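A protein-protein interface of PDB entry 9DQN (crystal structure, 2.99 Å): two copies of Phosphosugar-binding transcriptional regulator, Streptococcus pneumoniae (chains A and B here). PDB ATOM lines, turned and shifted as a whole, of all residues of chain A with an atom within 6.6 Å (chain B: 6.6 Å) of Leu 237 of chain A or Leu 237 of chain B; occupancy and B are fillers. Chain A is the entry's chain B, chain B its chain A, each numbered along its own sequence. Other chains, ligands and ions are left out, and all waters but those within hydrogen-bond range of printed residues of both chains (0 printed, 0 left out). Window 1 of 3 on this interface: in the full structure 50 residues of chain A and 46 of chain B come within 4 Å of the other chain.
N of Gln 236 of chain B sits close to OG of Ser 234 of chain B, 3.4 Å away.
N of Gln 236 of chain A lies close to OG of Ser 234 of chain A (3.3 Å).
The side-chain hydroxyl of Tyr 98 of chain B sits at hydrogen-bond distance from the backbone carbonyl oxygen of Leu 240 of chain A (2.7 Å).
OH of Tyr 98 of chain B lies within hydrogen-bond range of N of Phe 241 of chain A (3.4 Å).
OE2 of Glu 141 of chain A lies within hydrogen-bond range of OG of Ser 234 of chain B (2.5 Å).
N of Ser 234 of chain B is in hydrogen-bond range of OD1 of Asp 244 of chain A (3.1 Å).
OE2 of Glu 141 of chain A is in hydrogen-bond range of NE2 of Gln 236 of chain B, at 3.3 Å.
OE1 of Gln 236 of chain A lies close to OE1 of Gln 236 of chain B, at 2.9 Å.
O of Leu 240 of chain B sits at hydrogen-bond distance from OH of Tyr 98 of chain A (2.9 Å).
OH of Tyr 98 of chain A lies within hydrogen-bond range of N of Phe 241 of chain B (3.2 Å).
The side-chain hydroxyl of Tyr 98 of chain A lies within hydrogen-bond range of the side-chain carboxylate of Asp 244 of chain B, 2.9 Å away.
The backbone NH (N) of Ser 234 of chain A is in hydrogen-bond range of the side-chain carboxylate (OD2) of Asp 244 of chain B, at 3.0 Å.
The side-chain carboxylate of Asp 244 of chain A lies close to the side-chain hydroxyl of Tyr 98 of chain B, at 2.3 Å.
Tyr 98 of chain A touches Leu 240 of chain B, and with the chains exchanged Leu 240 of chain A touches Tyr 98 of chain B.
Tyr 98 of chain A touches Asp 244 of chain B, and with the chains exchanged Asp 244 of chain A touches Tyr 98 of chain B.
Ser 234 of chain A touches Asp 244 of chain B, and with the chains exchanged Asp 244 of chain A touches Ser 234 of chain B.
Leu 237 of chain A touches Leu 240 of chain B, and with the chains exchanged Leu 240 of chain A touches Leu 237 of chain B.
Of the 20 pairs that touch across the chains among the printed residues, 16 have their exchanged pair printed and touching as well.
Printed residues of chain B that touch a printed residue of chain A: Tyr 98, Ile 233, Ser 234, Ala 235, Gln 236, Leu 237, Leu 240, Phe 241 and Asp 244.
Hydrophobic or aromatic side chains of chain B that line the printed part of chain A: Tyr 98, Ile 233, Leu 237, Leu 240 and Phe 241.
Of the 18 printed residues of chain A, 9 touch a printed residue of chain B.
Among the printed residues, no Asp or Glu carboxylate lies within 4 Å of a Lys or Arg side-chain nitrogen of the other chain.
Among the printed residues, pairs that only touch across the chains: Glu 141 of chain A with Ala 235 of chain B (3.9 Å), Ile 233 of chain A with Asp 244 of chain B (3.3 Å), Ser 234 of chain A with Leu 240 of chain B (3.6 Å), Leu 237 of chain A with Leu 237 of chain B (3.9 Å), Leu 237 of chain A with Leu 240 of chain B (3.7 Å), Leu 237 of chain A with Asp 244 of chain B (3.98 Å), Leu 240 of chain A with Ser 234 of chain B (3.6 Å), Leu 240 of chain A with Leu 237 of chain B (3.9 Å) and Asp 244 of chain A with Ile 233 of chain B (3.6 Å).
Leu 237 of chain A touches three residues of chain B.
Thr 105 of chain B touches none of the printed residues of chain A.
Of the printed residues of chain A, Gln 236 of chain B touches Glu 141 (3.3 Å) and Gln 236 (2.9 Å).
Of the printed residues of chain A, Asp 244 of chain B touches Tyr 98 (2.9 Å), Ile 233 (3.3 Å), Ser 234 (3.0 Å) and Leu 237 (3.98 Å).
The nearest residue of chain B that does not touch Leu 237 of chain A is Tyr 98 of chain B (5.2 Å).
The nearest residue of chain A that does not touch Leu 237 of chain B is Tyr 98 of chain A (4.2 Å).
The nearest printed residue of chain B that does not touch Phe 241 of chain A is Leu 237 of chain B (6.3 Å).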
ATOM      1  N   SER A  97     -17.191  16.815 -16.054  1.00  0.00           N
ATOM      2  CA  SER A  97     -17.955  15.593 -15.833  1.00  0.00           C
ATOM      3  C   SER A  97     -17.070  14.356 -15.896  1.00  0.00           C
ATOM      4  O   SER A  97     -17.321  13.378 -15.181  1.00  0.00           O
ATOM      5  CB  SER A  97     -19.089  15.495 -16.853  1.00  0.00           C
ATOM      6  OG  SER A  97     -20.013  16.557 -16.693  1.00  0.00           O
ATOM      7  N   TYR A  98     -16.038  14.375 -16.742  1.00  0.00           N
ATOM      8  CA  TYR A  98     -15.094  13.263 -16.780  1.00  0.00           C
ATOM      9  C   TYR A  98     -14.306  13.166 -15.479  1.00  0.00           C
ATOM     10  O   TYR A  98     -14.214  12.092 -14.875  1.00  0.00           O
ATOM     11  CB  TYR A  98     -14.150  13.418 -17.972  1.00  0.00           C
ATOM     12  CG  TYR A  98     -14.651  12.775 -19.245  1.00  0.00           C
ATOM     13  CD1 TYR A  98     -15.399  13.498 -20.167  1.00  0.00           C
ATOM     14  CD2 TYR A  98     -14.374  11.444 -19.523  1.00  0.00           C
ATOM     15  CE1 TYR A  98     -15.856  12.908 -21.334  1.00  0.00           C
ATOM     16  CE2 TYR A  98     -14.822  10.849 -20.684  1.00  0.00           C
ATOM     17  CZ  TYR A  98     -15.564  11.582 -21.584  1.00  0.00           C
ATOM     18  OH  TYR A  98     -16.011  10.982 -22.736  1.00  0.00           O
ATOM     19  N   MET A 101     -16.526  12.284 -12.426  1.00  0.00           N
ATOM     20  CA  MET A 101     -16.830  10.858 -12.446  1.00  0.00           C
ATOM     21  C   MET A 101     -15.620  10.035 -12.027  1.00  0.00           C
ATOM     22  O   MET A 101     -15.758   9.022 -11.333  1.00  0.00           O
ATOM     23  CB  MET A 101     -17.311  10.442 -13.834  1.00  0.00           C
ATOM     24  CG  MET A 101     -17.650   8.971 -13.956  1.00  0.00           C
ATOM     25  SD  MET A 101     -18.861   8.690 -15.254  1.00  0.00           S
ATOM     26  CE  MET A 101     -20.171   9.778 -14.703  1.00  0.00           C
ATOM     27  N   THR A 105     -15.960   7.781  -8.878  1.00  0.00           N
ATOM     28  CA  THR A 105     -15.660   6.355  -8.999  1.00  0.00           C
ATOM     29  C   THR A 105     -14.547   5.956  -8.042  1.00  0.00           C
ATOM     30  O   THR A 105     -14.615   4.900  -7.399  1.00  0.00           O
ATOM     31  CB  THR A 105     -15.269   6.014 -10.440  1.00  0.00           C
ATOM     32  OG1 THR A 105     -16.441   5.962 -11.264  1.00  0.00           O
ATOM     33  CG2 THR A 105     -14.549   4.673 -10.507  1.00  0.00           C
ATOM     34  N   VAL A 138     -21.417  -1.459 -23.791  1.00  0.00           N
ATOM     35  CA  VAL A 138     -20.446  -1.816 -22.760  1.00  0.00           C
ATOM     36  C   VAL A 138     -20.245  -3.325 -22.726  1.00  0.00           C
ATOM     37  O   VAL A 138     -19.112  -3.815 -22.628  1.00  0.00           O
ATOM     38  CB  VAL A 138     -20.903  -1.268 -21.393  1.00  0.00           C
ATOM     39  CG1 VAL A 138     -20.332  -2.101 -20.255  1.00  0.00           C
ATOM     40  CG2 VAL A 138     -20.493   0.187 -21.245  1.00  0.00           C
ATOM     41  N   GLU A 141     -18.100  -4.433 -25.508  1.00  0.00           N
ATOM     42  CA  GLU A 141     -16.708  -4.081 -25.250  1.00  0.00           C
ATOM     43  C   GLU A 141     -16.012  -5.133 -24.383  1.00  0.00           C
ATOM     44  O   GLU A 141     -14.912  -5.584 -24.720  1.00  0.00           O
ATOM     45  CB  GLU A 141     -16.630  -2.699 -24.601  1.00  0.00           C
ATOM     46  CG  GLU A 141     -15.277  -2.365 -23.988  1.00  0.00           C
ATOM     47  CD  GLU A 141     -14.261  -1.878 -25.005  1.00  0.00           C
ATOM     48  OE1 GLU A 141     -14.045  -2.566 -26.027  1.00  0.00           O
ATOM     49  OE2 GLU A 141     -13.677  -0.797 -24.781  1.00  0.00           O
ATOM     50  N   HIS A 224     -23.617  10.419 -12.915  1.00  0.00           N
ATOM     51  CA  HIS A 224     -23.195  11.489 -13.807  1.00  0.00           C
ATOM     52  C   HIS A 224     -23.261  12.845 -13.111  1.00  0.00           C
ATOM     53  O   HIS A 224     -24.139  13.106 -12.285  1.00  0.00           O
ATOM     54  CB  HIS A 224     -24.052  11.499 -15.070  1.00  0.00           C
ATOM     55  CG  HIS A 224     -23.891  10.277 -15.920  1.00  0.00           C
ATOM     56  ND1 HIS A 224     -22.907  10.160 -16.878  1.00  0.00           N
ATOM     57  CD2 HIS A 224     -24.589   9.117 -15.953  1.00  0.00           C
ATOM     58  CE1 HIS A 224     -23.005   8.980 -17.465  1.00  0.00           C
ATOM     59  NE2 HIS A 224     -24.017   8.329 -16.922  1.00  0.00           N
ATOM     60  N   ILE A 233     -22.723  13.250 -19.870  1.00  0.00           N
ATOM     61  CA  ILE A 233     -21.731  12.691 -20.783  1.00  0.00           C
ATOM     62  C   ILE A 233     -22.101  11.250 -21.107  1.00  0.00           C
ATOM     63  O   ILE A 233     -23.195  10.787 -20.762  1.00  0.00           O
ATOM     64  CB  ILE A 233     -20.311  12.781 -20.194  1.00  0.00           C
ATOM     65  CG1 ILE A 233     -20.259  12.131 -18.808  1.00  0.00           C
ATOM     66  CG2 ILE A 233     -19.848  14.229 -20.138  1.00  0.00           C
ATOM     67  CD1 ILE A 233     -18.888  12.182 -18.154  1.00  0.00           C
ATOM     68  N   SER A 234     -21.198  10.541 -21.783  1.00  0.00           N
ATOM     69  CA  SER A 234     -21.471   9.179 -22.225  1.00  0.00           C
ATOM     70  C   SER A 234     -21.880   8.294 -21.056  1.00  0.00           C
ATOM     71  O   SER A 234     -21.235   8.290 -20.005  1.00  0.00           O
ATOM     72  CB  SER A 234     -20.235   8.597 -22.916  1.00  0.00           C
ATOM     73  OG  SER A 234     -20.406   7.218 -23.195  1.00  0.00           O
ATOM     74  N   ALA A 235     -22.967   7.543 -21.249  1.00  0.00           N
ATOM     75  CA  ALA A 235     -23.455   6.642 -20.213  1.00  0.00           C
ATOM     76  C   ALA A 235     -22.571   5.417 -20.030  1.00  0.00           C
ATOM     77  O   ALA A 235     -22.738   4.700 -19.037  1.00  0.00           O
ATOM     78  CB  ALA A 235     -24.884   6.200 -20.533  1.00  0.00           C
ATOM     79  N   GLN A 236     -21.648   5.154 -20.958  1.00  0.00           N
ATOM     80  CA  GLN A 236     -20.773   3.992 -20.825  1.00  0.00           C
ATOM     81  C   GLN A 236     -19.729   4.189 -19.736  1.00  0.00           C
ATOM     82  O   GLN A 236     -19.340   3.222 -19.070  1.00  0.00           O
ATOM     83  CB  GLN A 236     -20.073   3.700 -22.152  1.00  0.00           C
ATOM     84  CG  GLN A 236     -20.971   3.165 -23.258  1.00  0.00           C
ATOM     85  CD  GLN A 236     -20.170   2.702 -24.462  1.00  0.00           C
ATOM     86  OE1 GLN A 236     -19.189   1.967 -24.325  1.00  0.00           O
ATOM     87  NE2 GLN A 236     -20.577   3.140 -25.648  1.00  0.00           N
ATOM     88  N   LEU A 237     -19.281   5.428 -19.536  1.00  0.00           N
ATOM     89  CA  LEU A 237     -18.144   5.723 -18.664  1.00  0.00           C
ATOM     90  C   LEU A 237     -18.289   5.201 -17.238  1.00  0.00           C
ATOM     91  O   LEU A 237     -17.307   4.650 -16.716  1.00  0.00           O
ATOM     92  CB  LEU A 237     -17.903   7.238 -18.673  1.00  0.00           C
ATOM     93  CG  LEU A 237     -17.541   7.792 -20.050  1.00  0.00           C
ATOM     94  CD1 LEU A 237     -17.849   9.275 -20.116  1.00  0.00           C
ATOM     95  CD2 LEU A 237     -16.075   7.521 -20.363  1.00  0.00           C
ATOM     96  N   PRO A 238     -19.439   5.330 -16.553  1.00  0.00           N
ATOM     97  CA  PRO A 238     -19.503   4.830 -15.167  1.00  0.00           C
ATOM     98  C   PRO A 238     -19.113   3.366 -15.032  1.00  0.00           C
ATOM     99  O   PRO A 238     -18.489   2.993 -14.032  1.00  0.00           O
ATOM    100  CB  PRO A 238     -20.967   5.078 -14.782  1.00  0.00           C
ATOM    101  CG  PRO A 238     -21.377   6.237 -15.618  1.00  0.00           C
ATOM    102  CD  PRO A 238     -20.685   6.028 -16.932  1.00  0.00           C
ATOM    103  N   MET A 239     -19.441   2.529 -16.018  1.00  0.00           N
ATOM    104  CA  MET A 239     -19.047   1.125 -15.967  1.00  0.00           C
ATOM    105  C   MET A 239     -17.665   0.870 -16.554  1.00  0.00           C
ATOM    106  O   MET A 239     -16.976  -0.057 -16.111  1.00  0.00           O
ATOM    107  CB  MET A 239     -20.078   0.252 -16.691  1.00  0.00           C
ATOM    108  CG  MET A 239     -21.257  -0.154 -15.821  1.00  0.00           C
ATOM    109  SD  MET A 239     -22.696   0.923 -15.975  1.00  0.00           S
ATOM    110  CE  MET A 239     -23.419   0.295 -17.490  1.00  0.00           C
ATOM    111  N   LEU A 240     -17.237   1.675 -17.533  1.00  0.00           N
ATOM    112  CA  LEU A 240     -15.922   1.465 -18.137  1.00  0.00           C
ATOM    113  C   LEU A 240     -14.800   1.634 -17.121  1.00  0.00           C
ATOM    114  O   LEU A 240     -13.761   0.971 -17.233  1.00  0.00           O
ATOM    115  CB  LEU A 240     -15.719   2.414 -19.322  1.00  0.00           C
ATOM    116  CG  LEU A 240     -16.512   2.125 -20.602  1.00  0.00           C
ATOM    117  CD1 LEU A 240     -15.789   2.679 -21.825  1.00  0.00           C
ATOM    118  CD2 LEU A 240     -16.789   0.635 -20.763  1.00  0.00           C
ATOM    119  N   PHE A 241     -14.981   2.514 -16.131  1.00  0.00           N
ATOM    120  CA  PHE A 241     -14.004   2.623 -15.052  1.00  0.00           C
ATOM    121  C   PHE A 241     -13.819   1.284 -14.354  1.00  0.00           C
ATOM    122  O   PHE A 241     -12.690   0.811 -14.174  1.00  0.00           O
ATOM    123  CB  PHE A 241     -14.443   3.684 -14.041  1.00  0.00           C
ATOM    124  CG  PHE A 241     -14.106   5.091 -14.442  1.00  0.00           C
ATOM    125  CD1 PHE A 241     -12.889   5.651 -14.090  1.00  0.00           C
ATOM    126  CD2 PHE A 241     -15.012   5.859 -15.151  1.00  0.00           C
ATOM    127  CE1 PHE A 241     -12.580   6.951 -14.447  1.00  0.00           C
ATOM    128  CE2 PHE A 241     -14.711   7.158 -15.514  1.00  0.00           C
ATOM    129  CZ  PHE A 241     -13.493   7.706 -15.161  1.00  0.00           C
ATOM    130  N   PHE A 242     -14.926   0.650 -13.961  1.00  0.00           N
ATOM    131  CA  PHE A 242     -14.839  -0.651 -13.311  1.00  0.00           C
ATOM    132  C   PHE A 242     -14.509  -1.755 -14.307  1.00  0.00           C
ATOM    133  O   PHE A 242     -13.902  -2.763 -13.927  1.00  0.00           O
ATOM    134  CB  PHE A 242     -16.143  -0.951 -12.570  1.00  0.00           C
ATOM    135  CG  PHE A 242     -16.397  -0.038 -11.398  1.00  0.00           C
ATOM    136  CD1 PHE A 242     -16.991   1.201 -11.580  1.00  0.00           C
ATOM    137  CD2 PHE A 242     -16.035  -0.417 -10.115  1.00  0.00           C
ATOM    138  CE1 PHE A 242     -17.220   2.042 -10.506  1.00  0.00           C
ATOM    139  CE2 PHE A 242     -16.263   0.420  -9.037  1.00  0.00           C
ATOM    140  CZ  PHE A 242     -16.856   1.651  -9.233  1.00  0.00           C
ATOM    141  N   ASP A 244     -12.276  -1.577 -16.738  1.00  0.00           N
ATOM    142  CA  ASP A 244     -10.821  -1.624 -16.834  1.00  0.00           C
ATOM    143  C   ASP A 244     -10.182  -2.068 -15.524  1.00  0.00           C
ATOM    144  O   ASP A 244      -9.113  -2.689 -15.540  1.00  0.00           O
ATOM    145  CB  ASP A 244     -10.287  -0.257 -17.266  1.00  0.00           C
ATOM    146  CG  ASP A 244     -10.705   0.108 -18.680  1.00  0.00           C
ATOM    147  OD1 ASP A 244     -10.604  -0.758 -19.574  1.00  0.00           O
ATOM    148  OD2 ASP A 244     -11.144   1.255 -18.901  1.00  0.00           O
ATOM    149  N   TYR B  98      -6.777   6.709 -16.904  1.00  0.00           N
ATOM    150  CA  TYR B  98      -7.980   7.490 -17.171  1.00  0.00           C
ATOM    151  C   TYR B  98      -7.700   8.981 -17.064  1.00  0.00           C
ATOM    152  O   TYR B  98      -8.087   9.763 -17.941  1.00  0.00           O
ATOM    153  CB  TYR B  98      -9.093   7.085 -16.211  1.00  0.00           C
ATOM    154  CG  TYR B  98      -9.987   6.012 -16.767  1.00  0.00           C
ATOM    155  CD1 TYR B  98      -9.670   4.670 -16.616  1.00  0.00           C
ATOM    156  CD2 TYR B  98     -11.144   6.340 -17.456  1.00  0.00           C
ATOM    157  CE1 TYR B  98     -10.484   3.687 -17.129  1.00  0.00           C
ATOM    158  CE2 TYR B  98     -11.967   5.365 -17.971  1.00  0.00           C
ATOM    159  CZ  TYR B  98     -11.632   4.040 -17.806  1.00  0.00           C
ATOM    160  OH  TYR B  98     -12.453   3.068 -18.323  1.00  0.00           O
ATOM    161  N   MET B 101      -5.206  10.209 -19.896  1.00  0.00           N
ATOM    162  CA  MET B 101      -5.907  10.467 -21.150  1.00  0.00           C
ATOM    163  C   MET B 101      -6.636  11.803 -21.105  1.00  0.00           C
ATOM    164  O   MET B 101      -6.658  12.541 -22.096  1.00  0.00           O
ATOM    165  CB  MET B 101      -6.884   9.332 -21.447  1.00  0.00           C
ATOM    166  CG  MET B 101      -7.409   9.317 -22.870  1.00  0.00           C
ATOM    167  SD  MET B 101      -7.543   7.620 -23.441  1.00  0.00           S
ATOM    168  CE  MET B 101      -5.967   6.984 -22.868  1.00  0.00           C
ATOM    169  N   THR B 105      -6.055  14.913 -23.469  1.00  0.00           N
ATOM    170  CA  THR B 105      -7.190  15.329 -24.291  1.00  0.00           C
ATOM    171  C   THR B 105      -7.445  16.827 -24.174  1.00  0.00           C
ATOM    172  O   THR B 105      -7.712  17.497 -25.179  1.00  0.00           O
ATOM    173  CB  THR B 105      -8.442  14.538 -23.901  1.00  0.00           C
ATOM    174  OG1 THR B 105      -8.366  13.214 -24.447  1.00  0.00           O
ATOM    175  CG2 THR B 105      -9.702  15.218 -24.422  1.00  0.00           C
ATOM    176  N   VAL B 138     -17.926   2.970 -30.617  1.00  0.00           N
ATOM    177  CA  VAL B 138     -18.034   4.421 -30.484  1.00  0.00           C
ATOM    178  C   VAL B 138     -19.006   4.979 -31.515  1.00  0.00           C
ATOM    179  O   VAL B 138     -19.819   5.862 -31.212  1.00  0.00           O
ATOM    180  CB  VAL B 138     -16.649   5.079 -30.609  1.00  0.00           C
ATOM    181  CG1 VAL B 138     -16.799   6.588 -30.663  1.00  0.00           C
ATOM    182  CG2 VAL B 138     -15.754   4.663 -29.453  1.00  0.00           C
ATOM    183  N   ALA B 222      -6.563  11.571 -28.066  1.00  0.00           N
ATOM    184  CA  ALA B 222      -5.494  11.204 -27.151  1.00  0.00           C
ATOM    185  C   ALA B 222      -5.014   9.778 -27.415  1.00  0.00           C
ATOM    186  O   ALA B 222      -5.711   8.955 -28.013  1.00  0.00           O
ATOM    187  CB  ALA B 222      -5.959  11.341 -25.700  1.00  0.00           C
ATOM    188  N   HIS B 224      -3.124   6.173 -25.708  1.00  0.00           N
ATOM    189  CA  HIS B 224      -3.212   5.409 -24.473  1.00  0.00           C
ATOM    190  C   HIS B 224      -1.948   5.571 -23.634  1.00  0.00           C
ATOM    191  O   HIS B 224      -0.829   5.563 -24.154  1.00  0.00           O
ATOM    192  CB  HIS B 224      -3.474   3.936 -24.780  1.00  0.00           C
ATOM    193  CG  HIS B 224      -4.882   3.652 -25.208  1.00  0.00           C
ATOM    194  ND1 HIS B 224      -5.918   3.515 -24.308  1.00  0.00           N
ATOM    195  CD2 HIS B 224      -5.428   3.489 -26.436  1.00  0.00           C
ATOM    196  CE1 HIS B 224      -7.039   3.277 -24.964  1.00  0.00           C
ATOM    197  NE2 HIS B 224      -6.770   3.255 -26.256  1.00  0.00           N
ATOM    198  N   ILE B 233      -6.155   0.776 -21.233  1.00  0.00           N
ATOM    199  CA  ILE B 233      -7.559   0.877 -20.844  1.00  0.00           C
ATOM    200  C   ILE B 233      -8.443   0.804 -22.083  1.00  0.00           C
ATOM    201  O   ILE B 233      -7.959   0.535 -23.189  1.00  0.00           O
ATOM    202  CB  ILE B 233      -7.828   2.167 -20.048  1.00  0.00           C
ATOM    203  CG1 ILE B 233      -6.987   3.321 -20.597  1.00  0.00           C
ATOM    204  CG2 ILE B 233      -7.558   1.950 -18.565  1.00  0.00           C
ATOM    205  CD1 ILE B 233      -7.322   4.664 -19.985  1.00  0.00           C
ATOM    206  N   SER B 234      -9.744   1.027 -21.901  1.00  0.00           N
ATOM    207  CA  SER B 234     -10.700   0.892 -22.994  1.00  0.00           C
ATOM    208  C   SER B 234     -10.324   1.790 -24.167  1.00  0.00           C
ATOM    209  O   SER B 234     -10.004   2.969 -23.988  1.00  0.00           O
ATOM    210  CB  SER B 234     -12.107   1.231 -22.503  1.00  0.00           C
ATOM    211  OG  SER B 234     -13.028   1.269 -23.579  1.00  0.00           O
ATOM    212  N   ALA B 235     -10.368   1.224 -25.375  1.00  0.00           N
ATOM    213  CA  ALA B 235      -9.999   1.960 -26.579  1.00  0.00           C
ATOM    214  C   ALA B 235     -11.041   2.994 -26.983  1.00  0.00           C
ATOM    215  O   ALA B 235     -10.757   3.823 -27.856  1.00  0.00           O
ATOM    216  CB  ALA B 235      -9.762   0.990 -27.737  1.00  0.00           C
ATOM    217  N   GLN B 236     -12.230   2.966 -26.381  1.00  0.00           N
ATOM    218  CA  GLN B 236     -13.263   3.942 -26.703  1.00  0.00           C
ATOM    219  C   GLN B 236     -12.995   5.308 -26.086  1.00  0.00           C
ATOM    220  O   GLN B 236     -13.562   6.302 -26.553  1.00  0.00           O
ATOM    221  CB  GLN B 236     -14.633   3.438 -26.239  1.00  0.00           C
ATOM    222  CG  GLN B 236     -14.985   2.031 -26.705  1.00  0.00           C
ATOM    223  CD  GLN B 236     -16.407   1.639 -26.348  1.00  0.00           C
ATOM    224  OE1 GLN B 236     -17.336   2.436 -26.482  1.00  0.00           O
ATOM    225  NE2 GLN B 236     -16.584   0.405 -25.889  1.00  0.00           N
ATOM    226  N   LEU B 237     -12.144   5.380 -25.059  1.00  0.00           N
ATOM    227  CA  LEU B 237     -11.959   6.630 -24.322  1.00  0.00           C
ATOM    228  C   LEU B 237     -11.481   7.788 -25.189  1.00  0.00           C
ATOM    229  O   LEU B 237     -12.065   8.882 -25.085  1.00  0.00           O
ATOM    230  CB  LEU B 237     -11.008   6.395 -23.143  1.00  0.00           C
ATOM    231  CG  LEU B 237     -11.653   6.248 -21.763  1.00  0.00           C
ATOM    232  CD1 LEU B 237     -12.241   7.572 -21.300  1.00  0.00           C
ATOM    233  CD2 LEU B 237     -12.719   5.164 -21.785  1.00  0.00           C
ATOM    234  N   PRO B 238     -10.450   7.649 -26.038  1.00  0.00           N
ATOM    235  CA  PRO B 238     -10.035   8.809 -26.847  1.00  0.00           C
ATOM    236  C   PRO B 238     -11.149   9.357 -27.719  1.00  0.00           C
ATOM    237  O   PRO B 238     -11.258  10.578 -27.892  1.00  0.00           O
ATOM    238  CB  PRO B 238      -8.876   8.254 -27.686  1.00  0.00           C
ATOM    239  CG  PRO B 238      -8.357   7.110 -26.899  1.00  0.00           C
ATOM    240  CD  PRO B 238      -9.564   6.493 -26.266  1.00  0.00           C
ATOM    241  N   MET B 239     -11.989   8.483 -28.271  1.00  0.00           N
ATOM    242  CA  MET B 239     -13.124   8.960 -29.051  1.00  0.00           C
ATOM    243  C   MET B 239     -14.216   9.521 -28.147  1.00  0.00           C
ATOM    244  O   MET B 239     -14.809  10.561 -28.458  1.00  0.00           O
ATOM    245  CB  MET B 239     -13.663   7.831 -29.927  1.00  0.00           C
ATOM    246  CG  MET B 239     -12.601   7.147 -30.771  1.00  0.00           C
ATOM    247  SD  MET B 239     -11.533   8.328 -31.614  1.00  0.00           S
ATOM    248  CE  MET B 239     -10.405   7.225 -32.461  1.00  0.00           C
ATOM    249  N   LEU B 240     -14.470   8.862 -27.011  1.00  0.00           N
ATOM    250  CA  LEU B 240     -15.574   9.254 -26.137  1.00  0.00           C
ATOM    251  C   LEU B 240     -15.453  10.706 -25.688  1.00  0.00           C
ATOM    252  O   LEU B 240     -16.464  11.406 -25.554  1.00  0.00           O
ATOM    253  CB  LEU B 240     -15.638   8.327 -24.920  1.00  0.00           C
ATOM    254  CG  LEU B 240     -16.287   6.951 -25.091  1.00  0.00           C
ATOM    255  CD1 LEU B 240     -16.193   6.155 -23.799  1.00  0.00           C
ATOM    256  CD2 LEU B 240     -17.734   7.082 -25.531  1.00  0.00           C
ATOM    257  N   PHE B 241     -14.227  11.174 -25.442  1.00  0.00           N
ATOM    258  CA  PHE B 241     -14.031  12.562 -25.031  1.00  0.00           C
ATOM    259  C   PHE B 241     -14.561  13.529 -26.083  1.00  0.00           C
ATOM    260  O   PHE B 241     -15.288  14.478 -25.763  1.00  0.00           O
ATOM    261  CB  PHE B 241     -12.548  12.830 -24.773  1.00  0.00           C
ATOM    262  CG  PHE B 241     -12.096  12.486 -23.385  1.00  0.00           C
ATOM    263  CD1 PHE B 241     -12.225  13.404 -22.356  1.00  0.00           C
ATOM    264  CD2 PHE B 241     -11.528  11.255 -23.109  1.00  0.00           C
ATOM    265  CE1 PHE B 241     -11.805  13.097 -21.078  1.00  0.00           C
ATOM    266  CE2 PHE B 241     -11.105  10.941 -21.832  1.00  0.00           C
ATOM    267  CZ  PHE B 241     -11.244  11.863 -20.815  1.00  0.00           C
ATOM    268  N   PHE B 242     -14.209  13.300 -27.348  1.00  0.00           N
ATOM    269  CA  PHE B 242     -14.556  14.245 -28.402  1.00  0.00           C
ATOM    270  C   PHE B 242     -16.012  14.133 -28.837  1.00  0.00           C
ATOM    271  O   PHE B 242     -16.615  15.144 -29.218  1.00  0.00           O
ATOM    272  CB  PHE B 242     -13.616  14.061 -29.595  1.00  0.00           C
ATOM    273  CG  PHE B 242     -12.215  14.533 -29.329  1.00  0.00           C
ATOM    274  CD1 PHE B 242     -11.281  13.685 -28.757  1.00  0.00           C
ATOM    275  CD2 PHE B 242     -11.836  15.829 -29.637  1.00  0.00           C
ATOM    276  CE1 PHE B 242      -9.993  14.120 -28.503  1.00  0.00           C
ATOM    277  CE2 PHE B 242     -10.549  16.269 -29.385  1.00  0.00           C
ATOM    278  CZ  PHE B 242      -9.627  15.413 -28.818  1.00  0.00           C
ATOM    279  N   ASP B 244     -18.483  13.462 -26.850  1.00  0.00           N
ATOM    280  CA  ASP B 244     -19.225  14.185 -25.821  1.00  0.00           C
ATOM    281  C   ASP B 244     -19.081  15.692 -25.994  1.00  0.00           C
ATOM    282  O   ASP B 244     -20.037  16.444 -25.765  1.00  0.00           O
ATOM    283  CB  ASP B 244     -18.758  13.755 -24.428  1.00  0.00           C
ATOM    284  CG  ASP B 244     -19.198  12.344 -24.070  1.00  0.00           C
ATOM    285  OD1 ASP B 244     -19.950  11.729 -24.856  1.00  0.00           O
ATOM    286  OD2 ASP B 244     -18.790  11.849 -22.998  1.00  0.00           O
